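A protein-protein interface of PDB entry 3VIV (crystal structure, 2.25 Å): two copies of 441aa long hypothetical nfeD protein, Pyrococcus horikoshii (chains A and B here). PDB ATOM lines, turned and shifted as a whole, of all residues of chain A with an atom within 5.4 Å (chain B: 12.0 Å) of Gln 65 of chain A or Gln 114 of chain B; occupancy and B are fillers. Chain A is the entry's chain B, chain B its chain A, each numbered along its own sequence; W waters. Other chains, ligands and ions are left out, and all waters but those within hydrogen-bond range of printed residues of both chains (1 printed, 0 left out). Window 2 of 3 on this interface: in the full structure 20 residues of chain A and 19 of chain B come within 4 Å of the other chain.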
ATOM      1  N   TYR A  24      -5.861 -13.642  -4.456  1.00  0.00           N
ATOM      2  CA  TYR A  24      -4.678 -12.969  -3.923  1.00  0.00           C
ATOM      3  C   TYR A  24      -4.280 -11.787  -4.822  1.00  0.00           C
ATOM      4  O   TYR A  24      -4.039 -10.675  -4.342  1.00  0.00           O
ATOM      5  CB  TYR A  24      -3.481 -13.924  -3.752  1.00  0.00           C
ATOM      6  CG  TYR A  24      -2.251 -13.134  -3.397  1.00  0.00           C
ATOM      7  CD1 TYR A  24      -2.025 -12.754  -2.079  1.00  0.00           C
ATOM      8  CD2 TYR A  24      -1.372 -12.667  -4.386  1.00  0.00           C
ATOM      9  CE1 TYR A  24      -0.941 -11.989  -1.728  1.00  0.00           C
ATOM     10  CE2 TYR A  24      -0.280 -11.871  -4.041  1.00  0.00           C
ATOM     11  CZ  TYR A  24      -0.073 -11.551  -2.695  1.00  0.00           C
ATOM     12  OH  TYR A  24       0.983 -10.779  -2.288  1.00  0.00           O
ATOM     13  N   GLU A  35      -2.819   2.192  -1.424  1.00  0.00           N
ATOM     14  CA  GLU A  35      -1.601   2.610  -0.709  1.00  0.00           C
ATOM     15  C   GLU A  35      -0.883   3.720  -1.466  1.00  0.00           C
ATOM     16  O   GLU A  35      -0.385   4.679  -0.863  1.00  0.00           O
ATOM     17  CB  GLU A  35      -0.635   1.442  -0.517  1.00  0.00           C
ATOM     18  CG  GLU A  35      -1.048   0.420   0.531  1.00  0.00           C
ATOM     19  CD  GLU A  35      -0.206  -0.840   0.461  1.00  0.00           C
ATOM     20  OE1 GLU A  35       0.075  -1.304  -0.660  1.00  0.00           O
ATOM     21  OE2 GLU A  35       0.164  -1.377   1.520  1.00  0.00           O
ATOM     22  N   ASN A  58      -1.759 -16.141   2.294  1.00  0.00           N
ATOM     23  CA  ASN A  58      -1.122 -15.077   1.542  1.00  0.00           C
ATOM     24  C   ASN A  58      -1.917 -13.772   1.597  1.00  0.00           C
ATOM     25  O   ASN A  58      -1.338 -12.672   1.666  1.00  0.00           O
ATOM     26  CB  ASN A  58      -0.877 -15.509   0.100  1.00  0.00           C
ATOM     27  CG  ASN A  58       0.277 -16.501  -0.029  1.00  0.00           C
ATOM     28  OD1 ASN A  58       1.102 -16.654   0.879  1.00  0.00           O
ATOM     29  ND2 ASN A  58       0.343 -17.171  -1.168  1.00  0.00           N
ATOM     30  N   VAL A  60      -4.070 -12.879   4.067  1.00  0.00           N
ATOM     31  CA  VAL A  60      -3.986 -12.366   5.430  1.00  0.00           C
ATOM     32  C   VAL A  60      -2.650 -11.624   5.628  1.00  0.00           C
ATOM     33  O   VAL A  60      -2.613 -10.532   6.190  1.00  0.00           O
ATOM     34  CB  VAL A  60      -4.170 -13.522   6.464  1.00  0.00           C
ATOM     35  CG1 VAL A  60      -3.814 -13.086   7.879  1.00  0.00           C
ATOM     36  CG2 VAL A  60      -5.616 -14.061   6.391  1.00  0.00           C
ATOM     37  N   GLN A  61      -1.573 -12.227   5.139  1.00  0.00           N
ATOM     38  CA  GLN A  61      -0.242 -11.649   5.202  1.00  0.00           C
ATOM     39  C   GLN A  61      -0.166 -10.307   4.434  1.00  0.00           C
ATOM     40  O   GLN A  61       0.386  -9.320   4.944  1.00  0.00           O
ATOM     41  CB  GLN A  61       0.780 -12.670   4.669  1.00  0.00           C
ATOM     42  CG  GLN A  61       2.228 -12.227   4.685  1.00  0.00           C
ATOM     43  CD  GLN A  61       2.983 -12.659   5.921  1.00  0.00           C
ATOM     44  OE1 GLN A  61       2.550 -12.414   7.061  1.00  0.00           O
ATOM     45  NE2 GLN A  61       4.139 -13.291   5.708  1.00  0.00           N
ATOM     46  N   ARG A  62      -0.724 -10.273   3.226  1.00  0.00           N
ATOM     47  CA  ARG A  62      -0.781  -9.045   2.455  1.00  0.00           C
ATOM     48  C   ARG A  62      -1.527  -7.946   3.235  1.00  0.00           C
ATOM     49  O   ARG A  62      -1.121  -6.769   3.219  1.00  0.00           O
ATOM     50  CB  ARG A  62      -1.422  -9.281   1.089  1.00  0.00           C
ATOM     51  CG  ARG A  62      -1.503  -8.035   0.199  1.00  0.00           C
ATOM     52  CD  ARG A  62      -0.142  -7.576  -0.278  1.00  0.00           C
ATOM     53  NE  ARG A  62      -0.199  -6.328  -1.037  1.00  0.00           N
ATOM     54  CZ  ARG A  62      -0.010  -5.114  -0.510  1.00  0.00           C
ATOM     55  NH1 ARG A  62       0.230  -4.965   0.801  1.00  0.00           N
ATOM     56  NH2 ARG A  62      -0.057  -4.045  -1.290  1.00  0.00           N
ATOM     57  N   ILE A  63      -2.595  -8.333   3.930  1.00  0.00           N
ATOM     58  CA  ILE A  63      -3.353  -7.389   4.746  1.00  0.00           C
ATOM     59  C   ILE A  63      -2.552  -6.924   5.982  1.00  0.00           C
ATOM     60  O   ILE A  63      -2.627  -5.746   6.342  1.00  0.00           O
ATOM     61  CB  ILE A  63      -4.758  -7.939   5.113  1.00  0.00           C
ATOM     62  CG1 ILE A  63      -5.620  -8.056   3.845  1.00  0.00           C
ATOM     63  CG2 ILE A  63      -5.458  -7.045   6.172  1.00  0.00           C
ATOM     64  CD1 ILE A  63      -6.885  -8.879   4.001  1.00  0.00           C
ATOM     65  N   GLN A  64      -1.763  -7.812   6.602  1.00  0.00           N
ATOM     66  CA  GLN A  64      -0.877  -7.376   7.700  1.00  0.00           C
ATOM     67  C   GLN A  64       0.173  -6.373   7.247  1.00  0.00           C
ATOM     68  O   GLN A  64       0.598  -5.520   8.039  1.00  0.00           O
ATOM     69  CB  GLN A  64      -0.115  -8.526   8.379  1.00  0.00           C
ATOM     70  CG  GLN A  64      -0.828  -9.852   8.523  1.00  0.00           C
ATOM     71  CD  GLN A  64      -1.921  -9.851   9.552  1.00  0.00           C
ATOM     72  OE1 GLN A  64      -1.751 -10.395  10.639  1.00  0.00           O
ATOM     73  NE2 GLN A  64      -3.069  -9.289   9.204  1.00  0.00           N
ATOM     74  N   GLN A  65       0.622  -6.497   5.997  1.00  0.00           N
ATOM     75  CA  GLN A  65       1.720  -5.663   5.495  1.00  0.00           C
ATOM     76  C   GLN A  65       1.181  -4.351   4.919  1.00  0.00           C
ATOM     77  O   GLN A  65       1.957  -3.446   4.608  1.00  0.00           O
ATOM     78  CB  GLN A  65       2.584  -6.388   4.440  1.00  0.00           C
ATOM     79  CG  GLN A  65       3.209  -7.710   4.905  1.00  0.00           C
ATOM     80  CD  GLN A  65       3.676  -8.618   3.744  1.00  0.00           C
ATOM     81  OE1 GLN A  65       4.621  -9.397   3.910  1.00  0.00           O
ATOM     82  NE2 GLN A  65       3.026  -8.514   2.576  1.00  0.00           N
ATOM     83  N   SER A  66      -0.139  -4.273   4.777  1.00  0.00           N
ATOM     84  CA  SER A  66      -0.796  -3.111   4.208  1.00  0.00           C
ATOM     85  C   SER A  66      -0.494  -1.828   5.000  1.00  0.00           C
ATOM     86  O   SER A  66      -0.580  -1.788   6.239  1.00  0.00           O
ATOM     87  CB  SER A  66      -2.302  -3.319   4.144  1.00  0.00           C
ATOM     88  OG  SER A  66      -2.947  -2.135   3.679  1.00  0.00           O
ATOM     89  N   LYS A  67      -0.144  -0.792   4.260  1.00  0.00           N
ATOM     90  CA  LYS A  67       0.141   0.504   4.843  1.00  0.00           C
ATOM     91  C   LYS A  67      -1.156   1.304   5.053  1.00  0.00           C
ATOM     92  O   LYS A  67      -1.124   2.427   5.541  1.00  0.00           O
ATOM     93  CB  LYS A  67       1.184   1.234   3.986  1.00  0.00           C
ATOM     94  CG  LYS A  67       2.525   0.478   3.956  1.00  0.00           C
ATOM     95  CD  LYS A  67       3.531   1.065   2.977  1.00  0.00           C
ATOM     96  CE  LYS A  67       4.752   0.157   2.843  1.00  0.00           C
ATOM     97  NZ  LYS A  67       5.927   0.928   2.323  1.00  0.00           N
ATOM     98  N   ASN A 192       1.333  -0.473  10.136  1.00  0.00           N
ATOM     99  CA  ASN A 192       2.721  -0.113  10.418  1.00  0.00           C
ATOM    100  C   ASN A 192       2.956   0.131  11.915  1.00  0.00           C
ATOM    101  O   ASN A 192       3.386   1.214  12.322  1.00  0.00           O
ATOM    102  CB  ASN A 192       3.137   1.119   9.593  1.00  0.00           C
ATOM    103  CG  ASN A 192       3.971   0.760   8.350  1.00  0.00           C
ATOM    104  OD1 ASN A 192       4.956   1.444   8.041  1.00  0.00           O
ATOM    105  ND2 ASN A 192       3.579  -0.302   7.641  1.00  0.00           N
ATOM    106  N   ARG B  52      -3.336 -30.259  -6.936  1.00  0.00           N
ATOM    107  CA  ARG B  52      -4.025 -30.274  -5.658  1.00  0.00           C
ATOM    108  C   ARG B  52      -4.360 -31.709  -5.198  1.00  0.00           C
ATOM    109  O   ARG B  52      -4.723 -32.585  -6.008  1.00  0.00           O
ATOM    110  CB  ARG B  52      -5.273 -29.419  -5.762  1.00  0.00           C
ATOM    111  CG  ARG B  52      -4.991 -27.946  -6.122  1.00  0.00           C
ATOM    112  CD  ARG B  52      -4.984 -27.060  -4.857  1.00  0.00           C
ATOM    113  NE  ARG B  52      -4.270 -25.801  -5.067  1.00  0.00           N
ATOM    114  CZ  ARG B  52      -3.987 -24.923  -4.104  1.00  0.00           C
ATOM    115  NH1 ARG B  52      -3.323 -23.805  -4.392  1.00  0.00           N
ATOM    116  NH2 ARG B  52      -4.375 -25.164  -2.857  1.00  0.00           N
ATOM    117  N   ILE B 109       2.695 -30.330   0.579  1.00  0.00           N
ATOM    118  CA  ILE B 109       2.920 -28.985   1.131  1.00  0.00           C
ATOM    119  C   ILE B 109       1.592 -28.236   1.265  1.00  0.00           C
ATOM    120  O   ILE B 109       0.587 -28.577   0.607  1.00  0.00           O
ATOM    121  CB  ILE B 109       3.879 -28.125   0.257  1.00  0.00           C
ATOM    122  CG1 ILE B 109       3.289 -27.927  -1.145  1.00  0.00           C
ATOM    123  CG2 ILE B 109       5.271 -28.749   0.206  1.00  0.00           C
ATOM    124  CD1 ILE B 109       4.013 -26.908  -2.015  1.00  0.00           C
ATOM    125  N   LEU B 110       1.602 -27.219   2.124  1.00  0.00           N
ATOM    126  CA  LEU B 110       0.471 -26.327   2.255  1.00  0.00           C
ATOM    127  C   LEU B 110       0.445 -25.328   1.103  1.00  0.00           C
ATOM    128  O   LEU B 110      -0.601 -24.741   0.816  1.00  0.00           O
ATOM    129  CB  LEU B 110       0.446 -25.634   3.632  1.00  0.00           C
ATOM    130  CG  LEU B 110      -0.583 -26.170   4.646  1.00  0.00           C
ATOM    131  CD1 LEU B 110      -0.367 -25.584   6.048  1.00  0.00           C
ATOM    132  CD2 LEU B 110      -2.031 -25.920   4.174  1.00  0.00           C
ATOM    133  N   GLY B 111       1.585 -25.140   0.439  1.00  0.00           N
ATOM    134  CA  GLY B 111       1.633 -24.359  -0.801  1.00  0.00           C
ATOM    135  C   GLY B 111       2.770 -23.352  -0.854  1.00  0.00           C
ATOM    136  O   GLY B 111       3.882 -23.649  -0.421  1.00  0.00           O
ATOM    137  N   TYR B 112       2.476 -22.164  -1.379  1.00  0.00           N
ATOM    138  CA  TYR B 112       3.490 -21.144  -1.652  1.00  0.00           C
ATOM    139  C   TYR B 112       3.153 -19.764  -1.082  1.00  0.00           C
ATOM    140  O   TYR B 112       2.035 -19.283  -1.221  1.00  0.00           O
ATOM    141  CB  TYR B 112       3.712 -21.006  -3.163  1.00  0.00           C
ATOM    142  CG  TYR B 112       4.062 -22.296  -3.857  1.00  0.00           C
ATOM    143  CD1 TYR B 112       3.093 -23.008  -4.561  1.00  0.00           C
ATOM    144  CD2 TYR B 112       5.356 -22.816  -3.803  1.00  0.00           C
ATOM    145  CE1 TYR B 112       3.400 -24.198  -5.198  1.00  0.00           C
ATOM    146  CE2 TYR B 112       5.676 -24.016  -4.449  1.00  0.00           C
ATOM    147  CZ  TYR B 112       4.688 -24.695  -5.142  1.00  0.00           C
ATOM    148  OH  TYR B 112       4.973 -25.880  -5.782  1.00  0.00           O
ATOM    149  N   SER B 113       4.157 -19.140  -0.474  1.00  0.00           N
ATOM    150  CA  SER B 113       4.063 -17.795   0.077  1.00  0.00           C
ATOM    151  C   SER B 113       4.132 -16.723  -1.017  1.00  0.00           C
ATOM    152  O   SER B 113       4.311 -17.040  -2.193  1.00  0.00           O
ATOM    153  CB  SER B 113       5.172 -17.558   1.116  1.00  0.00           C
ATOM    154  OG  SER B 113       6.434 -17.405   0.487  1.00  0.00           O
ATOM    155  N   GLN B 114       3.997 -15.462  -0.605  1.00  0.00           N
ATOM    156  CA  GLN B 114       4.082 -14.315  -1.518  1.00  0.00           C
ATOM    157  C   GLN B 114       5.397 -14.320  -2.301  1.00  0.00           C
ATOM    158  O   GLN B 114       5.398 -14.114  -3.515  1.00  0.00           O
ATOM    159  CB  GLN B 114       3.916 -12.999  -0.758  1.00  0.00           C
ATOM    160  CG  GLN B 114       2.520 -12.768  -0.215  1.00  0.00           C
ATOM    161  CD  GLN B 114       2.448 -11.537   0.651  1.00  0.00           C
ATOM    162  OE1 GLN B 114       2.947 -11.531   1.769  1.00  0.00           O
ATOM    163  NE2 GLN B 114       1.833 -10.478   0.136  1.00  0.00           N
ATOM    164  N   ASN B 115       6.495 -14.561  -1.583  1.00  0.00           N
ATOM    165  CA  ASN B 115       7.811 -14.893  -2.147  1.00  0.00           C
ATOM    166  C   ASN B 115       7.789 -15.903  -3.286  1.00  0.00           C
ATOM    167  O   ASN B 115       8.575 -15.811  -4.224  1.00  0.00           O
ATOM    168  CB  ASN B 115       8.684 -15.514  -1.050  1.00  0.00           C
ATOM    169  CG  ASN B 115       9.765 -14.568  -0.554  1.00  0.00           C
ATOM    170  OD1 ASN B 115       9.886 -13.418  -1.013  1.00  0.00           O
ATOM    171  ND2 ASN B 115      10.569 -15.052   0.390  1.00  0.00           N
ATOM    172  N   GLY B 116       6.896 -16.882  -3.184  1.00  0.00           N
ATOM    173  CA  GLY B 116       7.021 -18.112  -3.951  1.00  0.00           C
ATOM    174  C   GLY B 116       7.787 -19.123  -3.110  1.00  0.00           C
ATOM    175  O   GLY B 116       8.172 -20.197  -3.600  1.00  0.00           O
ATOM    176  N   SER B 117       8.008 -18.773  -1.840  1.00  0.00           N
ATOM    177  CA  SER B 117       8.689 -19.649  -0.889  1.00  0.00           C
ATOM    178  C   SER B 117       7.819 -20.832  -0.510  1.00  0.00           C
ATOM    179  O   SER B 117       6.586 -20.763  -0.543  1.00  0.00           O
ATOM    180  CB  SER B 117       9.092 -18.904   0.387  1.00  0.00           C
ATOM    181  OG  SER B 117      10.213 -18.064   0.180  1.00  0.00           O
ATOM    182  N   ILE B 118       8.485 -21.905  -0.114  1.00  0.00           N
ATOM    183  CA  ILE B 118       7.834 -23.166   0.140  1.00  0.00           C
ATOM    184  C   ILE B 118       7.190 -23.166   1.528  1.00  0.00           C
ATOM    185  O   ILE B 118       7.848 -22.842   2.531  1.00  0.00           O
ATOM    186  CB  ILE B 118       8.863 -24.325  -0.051  1.00  0.00           C
ATOM    187  CG1 ILE B 118       8.183 -25.583  -0.587  1.00  0.00           C
ATOM    188  CG2 ILE B 118       9.782 -24.523   1.193  1.00  0.00           C
ATOM    189  CD1 ILE B 118       7.944 -25.506  -2.091  1.00  0.00           C
ATOM    190  N   ILE B 119       5.896 -23.482   1.585  1.00  0.00           N
ATOM    191  CA  ILE B 119       5.217 -23.632   2.878  1.00  0.00           C
ATOM    192  C   ILE B 119       4.961 -25.126   3.128  1.00  0.00           C
ATOM    193  O   ILE B 119       3.925 -25.663   2.705  1.00  0.00           O
ATOM    194  CB  ILE B 119       3.876 -22.834   2.975  1.00  0.00           C
ATOM    195  CG1 ILE B 119       4.019 -21.411   2.403  1.00  0.00           C
ATOM    196  CG2 ILE B 119       3.352 -22.817   4.427  1.00  0.00           C
ATOM    197  CD1 ILE B 119       2.698 -20.618   2.306  1.00  0.00           C
ATOM    198  N   GLU B 120       5.910 -25.786   3.806  1.00  0.00           N
ATOM    199  CA  GLU B 120       5.737 -27.187   4.217  1.00  0.00           C
ATOM    200  C   GLU B 120       4.557 -27.283   5.192  1.00  0.00           C
ATOM    201  O   GLU B 120       4.292 -26.351   5.962  1.00  0.00           O
ATOM    202  CB  GLU B 120       7.005 -27.765   4.885  1.00  0.00           C
ATOM    203  CG  GLU B 120       8.358 -27.339   4.302  1.00  0.00           C
ATOM    204  CD  GLU B 120       8.732 -28.037   2.999  1.00  0.00           C
ATOM    205  OE1 GLU B 120       7.911 -28.802   2.428  1.00  0.00           O
ATOM    206  OE2 GLU B 120       9.871 -27.809   2.536  1.00  0.00           O
HETATM  207  O   HOH W   1       4.123 -14.584   2.510  1.00  0.00           O
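Water W1 lies within hydrogen-bond range of the backbone NH (N) of Gln 114 of chain B (3.2 Å) and the side-chain amide nitrogen (NE2) of Gln 61 of chain A (3.4 Å).
Gln 65 of chain A touches one residue of chain B.
Of the printed residues of chain A, Gln 114 of chain B touches Tyr 24, Asn 58, Gln 61, Arg 62 and Gln 65.
Asn 58 of chain A touches just these residues of chain B: Tyr 112, Ser 113 and Gln 114.
Of chain B, only Gln 114 (3.5 Å) comes within 4 Å of Arg 62 of chain A.
No residue of chain B comes within 4 Å of Gln 64 of chain A.
No residue of chain B comes within 4 Å of Ser 66 of chain A.
No residue of chain B comes within 4 Å of Lys 67 of chain A.
Printed residues of chain A within 4 Å of Ser 113 of chain B: Asn 58 (3.3 Å).
Of the printed residues of chain B, Tyr 24 of chain A touches Gln 114.
Printed residues of chain A within 4 Å of Tyr 112 of chain B: Asn 58 (2.7 Å).
Asn 192 of chain A touches none of the printed residues of chain B.
The nearest residue of chain B that does not touch Gln 65 of chain A is Asn 115 of chain B (7.8 Å).
The nearest printed residue of chain A that does not touch Gln 114 of chain B is Ile 63 of chain A (6.2 Å).
The nearest printed residue of chain B that does not touch Tyr 24 of chain A is Asn 115 of chain B (6.7 Å).
The side-chain hydroxyl (OG) of Ser 113 of chain B sits close to the backbone NH (N) of Ser 117 of chain B (3.1 Å).
OE1 of Glu 35 of chain A lies within salt-bridge range of NH2 of Arg 62 of chain A, 2.8 Å away.
The side-chain amide nitrogen (ND2) of Asn 58 of chain A lies within hydrogen-bond range of the backbone carbonyl oxygen (O) of Tyr 112 of chain B.
The side-chain amide nitrogen of Gln 114 of chain B lies within hydrogen-bond range of the side-chain hydroxyl of Tyr 24 of chain A (2.6 Å).
The side-chain amide oxygen of Asn 58 of chain A lies within hydrogen-bond range of the backbone NH of Gln 114 of chain B (3.5 Å).
NE2 of Gln 65 of chain A lies within hydrogen-bond range of OE1 of Gln 114 of chain B.
Among the printed residues, pairs that only touch across the chains: Asn 58 of chain A with Ser 113 of chain B, Gln 61 of chain A with Gln 114 of chain B and Arg 62 of chain A with Gln 114 of chain B.
Of the 13 printed residues of chain B, 3 touch a printed residue of chain A.
Hydrophobic or aromatic side chains of chain A that line the printed part of chain B: Tyr 24.
Among the printed residues, 7 pairs touch across the chains.
No position is printed for both chains.
Of the 7 pairs that touch across the chains among the printed residues, none has its exchanged pair printed and touching as well.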
